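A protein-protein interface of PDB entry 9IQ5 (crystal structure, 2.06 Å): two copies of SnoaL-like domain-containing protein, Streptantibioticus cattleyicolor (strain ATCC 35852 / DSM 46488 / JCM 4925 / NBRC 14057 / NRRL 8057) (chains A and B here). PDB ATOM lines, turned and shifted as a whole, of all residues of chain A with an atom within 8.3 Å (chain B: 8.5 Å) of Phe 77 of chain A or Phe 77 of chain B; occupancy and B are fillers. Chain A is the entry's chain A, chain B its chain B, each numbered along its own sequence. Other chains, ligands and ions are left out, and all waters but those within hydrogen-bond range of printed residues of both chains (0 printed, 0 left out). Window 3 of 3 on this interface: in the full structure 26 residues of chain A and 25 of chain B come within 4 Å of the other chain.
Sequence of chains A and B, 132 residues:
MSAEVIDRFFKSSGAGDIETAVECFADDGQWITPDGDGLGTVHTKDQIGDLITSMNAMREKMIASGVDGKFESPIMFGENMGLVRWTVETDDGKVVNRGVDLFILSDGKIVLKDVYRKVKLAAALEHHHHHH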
ATOM      1  N   ILE A   6       1.435 -15.334  -9.007  1.00  0.00           N
ATOM      2  CA  ILE A   6       1.199 -15.709  -7.616  1.00  0.00           C
ATOM      3  C   ILE A   6       2.216 -15.022  -6.710  1.00  0.00           C
ATOM      4  O   ILE A   6       1.882 -14.499  -5.636  1.00  0.00           O
ATOM      5  CB  ILE A   6       1.230 -17.243  -7.453  1.00  0.00           C
ATOM      6  CG1 ILE A   6       0.130 -17.895  -8.284  1.00  0.00           C
ATOM      7  CG2 ILE A   6       1.023 -17.601  -5.980  1.00  0.00           C
ATOM      8  CD1 ILE A   6       0.122 -19.420  -8.256  1.00  0.00           C
ATOM      9  N   PRO A  74       4.883 -21.324  -4.248  1.00  0.00           N
ATOM     10  CA  PRO A  74       3.890 -22.117  -4.994  1.00  0.00           C
ATOM     11  C   PRO A  74       4.493 -23.373  -5.601  1.00  0.00           C
ATOM     12  O   PRO A  74       5.607 -23.364  -6.122  1.00  0.00           O
ATOM     13  CB  PRO A  74       3.430 -21.163  -6.103  1.00  0.00           C
ATOM     14  CG  PRO A  74       3.856 -19.784  -5.634  1.00  0.00           C
ATOM     15  CD  PRO A  74       5.063 -19.981  -4.825  1.00  0.00           C
ATOM     16  N   ILE A  75       3.721 -24.442  -5.576  1.00  0.00           N
ATOM     17  CA  ILE A  75       4.026 -25.662  -6.307  1.00  0.00           C
ATOM     18  C   ILE A  75       3.098 -25.681  -7.516  1.00  0.00           C
ATOM     19  O   ILE A  75       1.878 -25.803  -7.363  1.00  0.00           O
ATOM     20  CB  ILE A  75       3.815 -26.901  -5.427  1.00  0.00           C
ATOM     21  CG1 ILE A  75       4.755 -26.857  -4.205  1.00  0.00           C
ATOM     22  CG2 ILE A  75       3.999 -28.187  -6.268  1.00  0.00           C
ATOM     23  CD1 ILE A  75       4.433 -27.932  -3.149  1.00  0.00           C
ATOM     24  N   MET A  76       3.667 -25.528  -8.718  1.00  0.00           N
ATOM     25  CA  MET A  76       2.885 -25.445  -9.949  1.00  0.00           C
ATOM     26  C   MET A  76       2.577 -26.832 -10.498  1.00  0.00           C
ATOM     27  O   MET A  76       3.452 -27.712 -10.545  1.00  0.00           O
ATOM     28  CB  MET A  76       3.618 -24.619 -11.028  1.00  0.00           C
ATOM     29  CG  MET A  76       4.013 -23.179 -10.623  1.00  0.00           C
ATOM     30  SD  MET A  76       2.561 -22.201 -10.130  1.00  0.00           S
ATOM     31  CE  MET A  76       1.593 -22.218 -11.641  1.00  0.00           C
ATOM     32  N   PHE A  77       1.344 -27.002 -10.965  1.00  0.00           N
ATOM     33  CA  PHE A  77       0.943 -28.216 -11.684  1.00  0.00           C
ATOM     34  C   PHE A  77       0.487 -27.777 -13.079  1.00  0.00           C
ATOM     35  O   PHE A  77      -0.641 -27.311 -13.248  1.00  0.00           O
ATOM     36  CB  PHE A  77      -0.161 -28.942 -10.906  1.00  0.00           C
ATOM     37  CG  PHE A  77       0.290 -29.482  -9.566  1.00  0.00           C
ATOM     38  CD1 PHE A  77       0.851 -30.754  -9.464  1.00  0.00           C
ATOM     39  CD2 PHE A  77       0.179 -28.715  -8.420  1.00  0.00           C
ATOM     40  CE1 PHE A  77       1.271 -31.246  -8.232  1.00  0.00           C
ATOM     41  CE2 PHE A  77       0.591 -29.198  -7.187  1.00  0.00           C
ATOM     42  CZ  PHE A  77       1.134 -30.464  -7.094  1.00  0.00           C
ATOM     43  N   GLY A  78       1.339 -27.945 -14.079  1.00  0.00           N
ATOM     44  CA  GLY A  78       1.168 -27.247 -15.344  1.00  0.00           C
ATOM     45  C   GLY A  78       1.407 -25.745 -15.151  1.00  0.00           C
ATOM     46  O   GLY A  78       1.833 -25.280 -14.086  1.00  0.00           O
ATOM     47  N   GLU A  79       1.004 -24.976 -16.162  1.00  0.00           N
ATOM     48  CA  GLU A  79       1.206 -23.534 -16.151  1.00  0.00           C
ATOM     49  C   GLU A  79       0.094 -22.761 -15.453  1.00  0.00           C
ATOM     50  O   GLU A  79       0.334 -21.631 -15.009  1.00  0.00           O
ATOM     51  CB  GLU A  79       1.324 -23.008 -17.584  1.00  0.00           C
ATOM     52  CG  GLU A  79       2.573 -23.453 -18.344  1.00  0.00           C
ATOM     53  CD  GLU A  79       3.851 -22.929 -17.691  1.00  0.00           C
ATOM     54  OE1 GLU A  79       3.784 -21.861 -17.037  1.00  0.00           O
ATOM     55  OE2 GLU A  79       4.930 -23.555 -17.838  1.00  0.00           O
ATOM     56  N   ASN A  80      -1.099 -23.343 -15.320  1.00  0.00           N
ATOM     57  CA  ASN A  80      -2.284 -22.610 -14.897  1.00  0.00           C
ATOM     58  C   ASN A  80      -2.828 -23.058 -13.536  1.00  0.00           C
ATOM     59  O   ASN A  80      -3.948 -22.700 -13.172  1.00  0.00           O
ATOM     60  CB  ASN A  80      -3.360 -22.691 -15.987  1.00  0.00           C
ATOM     61  CG  ASN A  80      -2.898 -22.064 -17.298  1.00  0.00           C
ATOM     62  OD1 ASN A  80      -3.074 -22.625 -18.377  1.00  0.00           O
ATOM     63  ND2 ASN A  80      -2.247 -20.905 -17.197  1.00  0.00           N
ATOM     64  N   MET A  81      -2.047 -23.783 -12.742  1.00  0.00           N
ATOM     65  CA  MET A  81      -2.501 -24.154 -11.408  1.00  0.00           C
ATOM     66  C   MET A  81      -1.313 -24.140 -10.461  1.00  0.00           C
ATOM     67  O   MET A  81      -0.262 -24.693 -10.789  1.00  0.00           O
ATOM     68  CB  MET A  81      -3.152 -25.533 -11.424  1.00  0.00           C
ATOM     69  CG  MET A  81      -4.000 -25.825 -10.238  1.00  0.00           C
ATOM     70  SD  MET A  81      -3.079 -26.522  -8.866  1.00  0.00           S
ATOM     71  CE  MET A  81      -4.180 -26.030  -7.541  1.00  0.00           C
ATOM     72  N   GLY A  82      -1.470 -23.478  -9.324  1.00  0.00           N
ATOM     73  CA  GLY A  82      -0.446 -23.467  -8.290  1.00  0.00           C
ATOM     74  C   GLY A  82      -1.069 -23.763  -6.941  1.00  0.00           C
ATOM     75  O   GLY A  82      -2.206 -23.368  -6.668  1.00  0.00           O
ATOM     76  N   LEU A  83      -0.331 -24.489  -6.110  1.00  0.00           N
ATOM     77  CA  LEU A  83      -0.759 -24.821  -4.751  1.00  0.00           C
ATOM     78  C   LEU A  83       0.172 -24.163  -3.740  1.00  0.00           C
ATOM     79  O   LEU A  83       1.373 -24.443  -3.744  1.00  0.00           O
ATOM     80  CB  LEU A  83      -0.745 -26.333  -4.567  1.00  0.00           C
ATOM     81  CG  LEU A  83      -0.879 -26.880  -3.153  1.00  0.00           C
ATOM     82  CD1 LEU A  83      -2.327 -27.015  -2.819  1.00  0.00           C
ATOM     83  CD2 LEU A  83      -0.218 -28.257  -3.118  1.00  0.00           C
ATOM     84  N   VAL A  84      -0.377 -23.348  -2.834  1.00  0.00           N
ATOM     85  CA  VAL A  84       0.402 -22.709  -1.774  1.00  0.00           C
ATOM     86  C   VAL A  84       0.005 -23.361  -0.456  1.00  0.00           C
ATOM     87  O   VAL A  84      -1.146 -23.249  -0.011  1.00  0.00           O
ATOM     88  CB  VAL A  84       0.194 -21.188  -1.726  1.00  0.00           C
ATOM     89  CG1 VAL A  84       0.945 -20.571  -0.526  1.00  0.00           C
ATOM     90  CG2 VAL A  84       0.664 -20.544  -3.025  1.00  0.00           C
ATOM     91  N   ARG A  85       0.949 -24.076   0.155  1.00  0.00           N
ATOM     92  CA  ARG A  85       0.725 -24.609   1.487  1.00  0.00           C
ATOM     93  C   ARG A  85       1.035 -23.538   2.522  1.00  0.00           C
ATOM     94  O   ARG A  85       2.016 -22.788   2.391  1.00  0.00           O
ATOM     95  CB  ARG A  85       1.599 -25.846   1.723  1.00  0.00           C
ATOM     96  CG  ARG A  85       1.489 -26.923   0.600  1.00  0.00           C
ATOM     97  CD  ARG A  85       2.076 -28.278   1.015  1.00  0.00           C
ATOM     98  NE  ARG A  85       1.114 -28.885   1.925  1.00  0.00           N
ATOM     99  CZ  ARG A  85       0.200 -29.795   1.601  1.00  0.00           C
ATOM    100  NH1 ARG A  85       0.201 -30.392   0.415  1.00  0.00           N
ATOM    101  NH2 ARG A  85      -0.786 -30.058   2.467  1.00  0.00           N
ATOM    102  N   LEU A 102      -5.419 -22.663  -3.197  1.00  0.00           N
ATOM    103  CA  LEU A 102      -5.450 -23.168  -4.554  1.00  0.00           C
ATOM    104  C   LEU A 102      -5.567 -21.987  -5.493  1.00  0.00           C
ATOM    105  O   LEU A 102      -6.534 -21.224  -5.402  1.00  0.00           O
ATOM    106  CB  LEU A 102      -6.651 -24.092  -4.749  1.00  0.00           C
ATOM    107  CG  LEU A 102      -6.342 -25.568  -4.614  1.00  0.00           C
ATOM    108  CD1 LEU A 102      -5.437 -25.861  -3.440  1.00  0.00           C
ATOM    109  CD2 LEU A 102      -7.647 -26.331  -4.523  1.00  0.00           C
ATOM    110  N   PHE A 103      -4.602 -21.825  -6.381  1.00  0.00           N
ATOM    111  CA  PHE A 103      -4.631 -20.747  -7.356  1.00  0.00           C
ATOM    112  C   PHE A 103      -4.866 -21.339  -8.730  1.00  0.00           C
ATOM    113  O   PHE A 103      -4.051 -22.137  -9.210  1.00  0.00           O
ATOM    114  CB  PHE A 103      -3.326 -19.958  -7.366  1.00  0.00           C
ATOM    115  CG  PHE A 103      -3.129 -19.060  -6.185  1.00  0.00           C
ATOM    116  CD1 PHE A 103      -2.618 -19.548  -4.996  1.00  0.00           C
ATOM    117  CD2 PHE A 103      -3.404 -17.711  -6.282  1.00  0.00           C
ATOM    118  CE1 PHE A 103      -2.394 -18.687  -3.905  1.00  0.00           C
ATOM    119  CE2 PHE A 103      -3.163 -16.842  -5.239  1.00  0.00           C
ATOM    120  CZ  PHE A 103      -2.673 -17.319  -4.030  1.00  0.00           C
ATOM    121  N   ILE A 104      -5.931 -20.901  -9.393  1.00  0.00           N
ATOM    122  CA  ILE A 104      -6.185 -21.245 -10.787  1.00  0.00           C
ATOM    123  C   ILE A 104      -5.898 -19.998 -11.616  1.00  0.00           C
ATOM    124  O   ILE A 104      -6.460 -18.932 -11.337  1.00  0.00           O
ATOM    125  CB  ILE A 104      -7.634 -21.716 -11.022  1.00  0.00           C
ATOM    126  CG1 ILE A 104      -8.056 -22.804 -10.019  1.00  0.00           C
ATOM    127  CG2 ILE A 104      -7.753 -22.267 -12.420  1.00  0.00           C
ATOM    128  CD1 ILE A 104      -7.250 -24.103 -10.165  1.00  0.00           C
ATOM    129  N   LEU A 105      -5.056 -20.135 -12.637  1.00  0.00           N
ATOM    130  CA  LEU A 105      -4.612 -19.024 -13.475  1.00  0.00           C
ATOM    131  C   LEU A 105      -5.144 -19.136 -14.896  1.00  0.00           C
ATOM    132  O   LEU A 105      -5.375 -20.236 -15.405  1.00  0.00           O
ATOM    133  CB  LEU A 105      -3.077 -18.934 -13.535  1.00  0.00           C
ATOM    134  CG  LEU A 105      -2.296 -19.063 -12.215  1.00  0.00           C
ATOM    135  CD1 LEU A 105      -0.765 -18.991 -12.476  1.00  0.00           C
ATOM    136  CD2 LEU A 105      -2.713 -17.992 -11.226  1.00  0.00           C
ATOM    137  N   LEU A 112      -8.966 -17.884  -9.846  1.00  0.00           N
ATOM    138  CA  LEU A 112      -9.522 -18.361  -8.585  1.00  0.00           C
ATOM    139  C   LEU A 112      -8.418 -18.481  -7.552  1.00  0.00           C
ATOM    140  O   LEU A 112      -7.357 -19.040  -7.842  1.00  0.00           O
ATOM    141  CB  LEU A 112     -10.218 -19.712  -8.774  1.00  0.00           C
ATOM    142  CG  LEU A 112     -10.747 -20.422  -7.527  1.00  0.00           C
ATOM    143  CD1 LEU A 112     -11.648 -19.502  -6.743  1.00  0.00           C
ATOM    144  CD2 LEU A 112     -11.531 -21.672  -7.956  1.00  0.00           C
ATOM    145  N   ILE B   6      -7.908 -42.431 -10.191  1.00  0.00           N
ATOM    146  CA  ILE B   6      -8.881 -41.714  -9.376  1.00  0.00           C
ATOM    147  C   ILE B   6     -10.290 -42.227  -9.660  1.00  0.00           C
ATOM    148  O   ILE B   6     -11.087 -42.473  -8.740  1.00  0.00           O
ATOM    149  CB  ILE B   6      -8.770 -40.207  -9.627  1.00  0.00           C
ATOM    150  CG1 ILE B   6      -7.336 -39.734  -9.358  1.00  0.00           C
ATOM    151  CG2 ILE B   6      -9.747 -39.487  -8.721  1.00  0.00           C
ATOM    152  CD1 ILE B   6      -7.115 -38.308  -9.709  1.00  0.00           C
ATOM    153  N   PRO B  74     -12.716 -35.873 -11.641  1.00  0.00           N
ATOM    154  CA  PRO B  74     -11.426 -35.223 -11.380  1.00  0.00           C
ATOM    155  C   PRO B  74     -11.068 -34.264 -12.501  1.00  0.00           C
ATOM    156  O   PRO B  74     -11.357 -34.505 -13.672  1.00  0.00           O
ATOM    157  CB  PRO B  74     -10.433 -36.391 -11.317  1.00  0.00           C
ATOM    158  CG  PRO B  74     -11.268 -37.607 -11.142  1.00  0.00           C
ATOM    159  CD  PRO B  74     -12.570 -37.327 -11.821  1.00  0.00           C
ATOM    160  N   ILE B  75     -10.480 -33.150 -12.115  1.00  0.00           N
ATOM    161  CA  ILE B  75      -9.875 -32.185 -13.024  1.00  0.00           C
ATOM    162  C   ILE B  75      -8.363 -32.291 -12.871  1.00  0.00           C
ATOM    163  O   ILE B  75      -7.819 -32.001 -11.799  1.00  0.00           O
ATOM    164  CB  ILE B  75     -10.394 -30.768 -12.745  1.00  0.00           C
ATOM    165  CG1 ILE B  75     -11.911 -30.750 -13.004  1.00  0.00           C
ATOM    166  CG2 ILE B  75      -9.684 -29.757 -13.593  1.00  0.00           C
ATOM    167  CD1 ILE B  75     -12.584 -29.461 -12.606  1.00  0.00           C
ATOM    168  N   MET B  76      -7.688 -32.741 -13.926  1.00  0.00           N
ATOM    169  CA  MET B  76      -6.244 -32.944 -13.879  1.00  0.00           C
ATOM    170  C   MET B  76      -5.514 -31.639 -14.188  1.00  0.00           C
ATOM    171  O   MET B  76      -5.919 -30.867 -15.063  1.00  0.00           O
ATOM    172  CB  MET B  76      -5.826 -34.022 -14.872  1.00  0.00           C
ATOM    173  CG  MET B  76      -6.652 -35.304 -14.753  1.00  0.00           C
ATOM    174  SD  MET B  76      -6.635 -36.122 -13.142  1.00  0.00           S
ATOM    175  CE  MET B  76      -4.884 -36.516 -13.006  1.00  0.00           C
ATOM    176  N   PHE B  77      -4.457 -31.374 -13.436  1.00  0.00           N
ATOM    177  CA  PHE B  77      -3.572 -30.241 -13.684  1.00  0.00           C
ATOM    178  C   PHE B  77      -2.168 -30.787 -13.868  1.00  0.00           C
ATOM    179  O   PHE B  77      -1.581 -31.329 -12.928  1.00  0.00           O
ATOM    180  CB  PHE B  77      -3.651 -29.237 -12.555  1.00  0.00           C
ATOM    181  CG  PHE B  77      -4.981 -28.571 -12.439  1.00  0.00           C
ATOM    182  CD1 PHE B  77      -5.235 -27.386 -13.098  1.00  0.00           C
ATOM    183  CD2 PHE B  77      -5.982 -29.127 -11.671  1.00  0.00           C
ATOM    184  CE1 PHE B  77      -6.441 -26.743 -12.974  1.00  0.00           C
ATOM    185  CE2 PHE B  77      -7.200 -28.489 -11.548  1.00  0.00           C
ATOM    186  CZ  PHE B  77      -7.431 -27.292 -12.204  1.00  0.00           C
ATOM    187  N   GLY B  78      -1.664 -30.735 -15.093  1.00  0.00           N
ATOM    188  CA  GLY B  78      -0.522 -31.594 -15.285  1.00  0.00           C
ATOM    189  C   GLY B  78      -1.038 -33.021 -15.214  1.00  0.00           C
ATOM    190  O   GLY B  78      -2.241 -33.281 -15.302  1.00  0.00           O
ATOM    191  N   GLU B  79      -0.112 -33.963 -15.060  1.00  0.00           N
ATOM    192  CA  GLU B  79      -0.500 -35.368 -15.081  1.00  0.00           C
ATOM    193  C   GLU B  79      -0.638 -36.013 -13.699  1.00  0.00           C
ATOM    194  O   GLU B  79      -1.328 -37.035 -13.582  1.00  0.00           O
ATOM    195  CB  GLU B  79       0.501 -36.168 -15.919  1.00  0.00           C
ATOM    196  CG  GLU B  79       0.734 -35.571 -17.317  1.00  0.00           C
ATOM    197  CD  GLU B  79      -0.547 -35.334 -18.121  1.00  0.00           C
ATOM    198  OE1 GLU B  79      -1.575 -36.014 -17.880  1.00  0.00           O
ATOM    199  OE2 GLU B  79      -0.515 -34.444 -19.006  1.00  0.00           O
ATOM    200  N   ASN B  80      -0.003 -35.459 -12.655  1.00  0.00           N
ATOM    201  CA  ASN B  80       0.134 -36.146 -11.371  1.00  0.00           C
ATOM    202  C   ASN B  80      -0.692 -35.501 -10.275  1.00  0.00           C
ATOM    203  O   ASN B  80      -0.527 -35.824  -9.097  1.00  0.00           O
ATOM    204  CB  ASN B  80       1.595 -36.194 -10.938  1.00  0.00           C
ATOM    205  CG  ASN B  80       2.463 -36.928 -11.922  1.00  0.00           C
ATOM    206  OD1 ASN B  80       3.530 -36.441 -12.299  1.00  0.00           O
ATOM    207  ND2 ASN B  80       2.018 -38.112 -12.347  1.00  0.00           N
ATOM    208  N   MET B  81      -1.627 -34.654 -10.649  1.00  0.00           N
ATOM    209  CA  MET B  81      -2.473 -34.001  -9.684  1.00  0.00           C
ATOM    210  C   MET B  81      -3.893 -33.970 -10.232  1.00  0.00           C
ATOM    211  O   MET B  81      -4.097 -33.705 -11.423  1.00  0.00           O
ATOM    212  CB  MET B  81      -1.931 -32.607  -9.397  1.00  0.00           C
ATOM    213  CG  MET B  81      -2.488 -32.009  -8.168  1.00  0.00           C
ATOM    214  SD  MET B  81      -3.962 -31.142  -8.624  1.00  0.00           S
ATOM    215  CE  MET B  81      -4.841 -31.202  -7.075  1.00  0.00           C
ATOM    216  N   GLY B  82      -4.848 -34.340  -9.390  1.00  0.00           N
ATOM    217  CA  GLY B  82      -6.256 -34.276  -9.751  1.00  0.00           C
ATOM    218  C   GLY B  82      -7.039 -33.593  -8.651  1.00  0.00           C
ATOM    219  O   GLY B  82      -6.762 -33.781  -7.467  1.00  0.00           O
ATOM    220  N   LEU B  83      -8.012 -32.789  -9.053  1.00  0.00           N
ATOM    221  CA  LEU B  83      -8.829 -32.021  -8.124  1.00  0.00           C
ATOM    222  C   LEU B  83     -10.258 -32.535  -8.232  1.00  0.00           C
ATOM    223  O   LEU B  83     -10.831 -32.518  -9.321  1.00  0.00           O
ATOM    224  CB  LEU B  83      -8.757 -30.533  -8.468  1.00  0.00           C
ATOM    225  CG  LEU B  83      -9.680 -29.553  -7.760  1.00  0.00           C
ATOM    226  CD1 LEU B  83      -8.979 -29.028  -6.515  1.00  0.00           C
ATOM    227  CD2 LEU B  83     -10.137 -28.417  -8.677  1.00  0.00           C
ATOM    228  N   VAL B  84     -10.817 -33.022  -7.127  1.00  0.00           N
ATOM    229  CA  VAL B  84     -12.206 -33.481  -7.074  1.00  0.00           C
ATOM    230  C   VAL B  84     -12.966 -32.546  -6.144  1.00  0.00           C
ATOM    231  O   VAL B  84     -12.678 -32.488  -4.942  1.00  0.00           O
ATOM    232  CB  VAL B  84     -12.313 -34.947  -6.618  1.00  0.00           C
ATOM    233  CG1 VAL B  84     -13.787 -35.380  -6.484  1.00  0.00           C
ATOM    234  CG2 VAL B  84     -11.637 -35.863  -7.610  1.00  0.00           C
ATOM    235  N   ARG B  85     -13.907 -31.778  -6.694  1.00  0.00           N
ATOM    236  CA  ARG B  85     -14.797 -30.962  -5.867  1.00  0.00           C
ATOM    237  C   ARG B  85     -15.984 -31.789  -5.385  1.00  0.00           C
ATOM    238  O   ARG B  85     -16.491 -32.670  -6.098  1.00  0.00           O
ATOM    239  CB  ARG B  85     -15.276 -29.727  -6.635  1.00  0.00           C
ATOM    240  CG  ARG B  85     -14.099 -28.931  -7.243  1.00  0.00           C
ATOM    241  CD  ARG B  85     -14.461 -27.577  -7.847  1.00  0.00           C
ATOM    242  NE  ARG B  85     -14.730 -26.542  -6.865  1.00  0.00           N
ATOM    243  CZ  ARG B  85     -13.834 -25.661  -6.427  1.00  0.00           C
ATOM    244  NH1 ARG B  85     -12.609 -25.597  -6.935  1.00  0.00           N
ATOM    245  NH2 ARG B  85     -14.184 -24.799  -5.473  1.00  0.00           N
ATOM    246  N   LEU B 102      -7.751 -33.372  -2.891  1.00  0.00           N
ATOM    247  CA  LEU B 102      -6.547 -33.201  -3.689  1.00  0.00           C
ATOM    248  C   LEU B 102      -5.873 -34.555  -3.813  1.00  0.00           C
ATOM    249  O   LEU B 102      -5.510 -35.153  -2.797  1.00  0.00           O
ATOM    250  CB  LEU B 102      -5.600 -32.220  -3.007  1.00  0.00           C
ATOM    251  CG  LEU B 102      -5.685 -30.767  -3.445  1.00  0.00           C
ATOM    252  CD1 LEU B 102      -7.107 -30.345  -3.640  1.00  0.00           C
ATOM    253  CD2 LEU B 102      -5.039 -29.896  -2.378  1.00  0.00           C
ATOM    254  N   PHE B 103      -5.688 -35.031  -5.042  1.00  0.00           N
ATOM    255  CA  PHE B 103      -5.031 -36.303  -5.313  1.00  0.00           C
ATOM    256  C   PHE B 103      -3.667 -36.060  -5.958  1.00  0.00           C
ATOM    257  O   PHE B 103      -3.581 -35.370  -6.982  1.00  0.00           O
ATOM    258  CB  PHE B 103      -5.871 -37.170  -6.253  1.00  0.00           C
ATOM    259  CG  PHE B 103      -7.125 -37.737  -5.639  1.00  0.00           C
ATOM    260  CD1 PHE B 103      -8.292 -36.991  -5.601  1.00  0.00           C
ATOM    261  CD2 PHE B 103      -7.146 -39.037  -5.147  1.00  0.00           C
ATOM    262  CE1 PHE B 103      -9.448 -37.532  -5.078  1.00  0.00           C
ATOM    263  CE2 PHE B 103      -8.299 -39.573  -4.602  1.00  0.00           C
ATOM    264  CZ  PHE B 103      -9.450 -38.831  -4.580  1.00  0.00           C
ATOM    265  N   ILE B 104      -2.608 -36.619  -5.367  1.00  0.00           N
ATOM    266  CA  ILE B 104      -1.271 -36.623  -5.955  1.00  0.00           C
ATOM    267  C   ILE B 104      -0.918 -38.047  -6.350  1.00  0.00           C
ATOM    268  O   ILE B 104      -0.971 -38.958  -5.515  1.00  0.00           O
ATOM    269  CB  ILE B 104      -0.220 -36.041  -4.988  1.00  0.00           C
ATOM    270  CG1 ILE B 104      -0.659 -34.669  -4.495  1.00  0.00           C
ATOM    271  CG2 ILE B 104       1.159 -35.992  -5.651  1.00  0.00           C
ATOM    272  CD1 ILE B 104      -0.779 -33.673  -5.596  1.00  0.00           C
ATOM    273  N   LEU B 105      -0.527 -38.235  -7.615  1.00  0.00           N
ATOM    274  CA  LEU B 105      -0.256 -39.547  -8.187  1.00  0.00           C
ATOM    275  C   LEU B 105       1.220 -39.683  -8.539  1.00  0.00           C
ATOM    276  O   LEU B 105       1.872 -38.709  -8.910  1.00  0.00           O
ATOM    277  CB  LEU B 105      -1.092 -39.757  -9.454  1.00  0.00           C
ATOM    278  CG  LEU B 105      -2.520 -39.223  -9.283  1.00  0.00           C
ATOM    279  CD1 LEU B 105      -3.327 -39.365 -10.566  1.00  0.00           C
ATOM    280  CD2 LEU B 105      -3.196 -39.947  -8.136  1.00  0.00           C
ATOM    281  N   LEU B 112      -1.046 -39.223  -2.426  1.00  0.00           N
ATOM    282  CA  LEU B 112      -1.689 -38.391  -1.428  1.00  0.00           C
ATOM    283  C   LEU B 112      -3.146 -38.170  -1.806  1.00  0.00           C
ATOM    284  O   LEU B 112      -3.458 -37.809  -2.945  1.00  0.00           O
ATOM    285  CB  LEU B 112      -0.978 -37.041  -1.290  1.00  0.00           C
ATOM    286  CG  LEU B 112      -1.642 -36.068  -0.324  1.00  0.00           C
ATOM    287  CD1 LEU B 112      -1.781 -36.717   1.040  1.00  0.00           C
ATOM    288  CD2 LEU B 112      -0.853 -34.766  -0.212  1.00  0.00           C
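Of the 18 printed residues of chain B, 4 touch a printed residue of chain A.
Hydrophobic or aromatic side chains of chain B within 4 Å of the printed part of chain A: Phe 77, Met 81, Leu 83 and Leu 102.
Of the 18 printed residues of chain A, 5 touch a printed residue of chain B.
Among the printed residues, 6 pairs touch across the chains.
Among the printed residues, no Asp or Glu carboxylate lies within 4 Å of a Lys or Arg side-chain nitrogen of the other chain.
Of the printed residues of chain B, Phe 77 of chain A touches Phe 77 and Met 81.
Of chain A, only Phe 77 (3.4 Å), Met 81 (3.3 Å) and Ile 104 (3.8 Å) come within 4 Å of Phe 77 of chain B.
No residue of chain B comes within 4 Å of Gly 78 of chain A.
No residue of chain A comes within 4 Å of Gly 78 of chain B.
Of the printed residues of chain B, Ile 104 of chain A touches Phe 77 (3.8 Å).
Of the printed residues of chain A, Leu 102 of chain B touches Leu 83.
Printed residues of chain A within 4 Å of Leu 83 of chain B: Leu 102 (3.6 Å).
Arg 85 of chain B touches none of the printed residues of chain A.
The nearest residue of chain A that does not touch Phe 77 of chain B is Gly 78 of chain A (4.5 Å).
Phe 77 of chain B touches its own counterpart, Phe 77 of chain A.
Phe 77 of chain A touches Met 81 of chain B, and with the chains exchanged Met 81 of chain A touches Phe 77 of chain B.
Leu 83 of chain A touches Leu 102 of chain B, and with the chains exchanged Leu 102 of chain A touches Leu 83 of chain B.
Ile 104 of chain A touches Phe 77 of chain B, but with the chains exchanged Phe 77 of chain A does not touch Ile 104 of chain B (4.03 Å).
18 positions are printed for both chains.
The backbone NH of Leu 83 of chain B lies within hydrogen-bond range of the backbone carbonyl oxygen of Ile 75 of chain B (2.9 Å).
The backbone carbonyl oxygen (O) of Ile 75 of chain A is in hydrogen-bond range of the backbone NH (N) of Leu 83 of chain A (2.9 Å).
The backbone carbonyl oxygen (O) of Leu 112 of chain A sits at hydrogen-bond distance from the backbone NH (N) of Ile 104 of chain A (2.8 Å).
CB of Phe 77 of chain A touches O of Phe 77 of chain B, at 3.4 Å.
Met 81 of chain B touches Phe 77 of chain A.
Phe 77 of chain B touches Met 81 of chain A (CD1 to CB, 3.3 Å).
CD2 of Leu 102 of chain B touches CD1 of Leu 83 of chain A, at 3.98 Å.
Leu 83 of chain B touches Leu 102 of chain A (CD1 to CD2, 3.6 Å).
Ile 104 of chain A touches Phe 77 of chain B.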
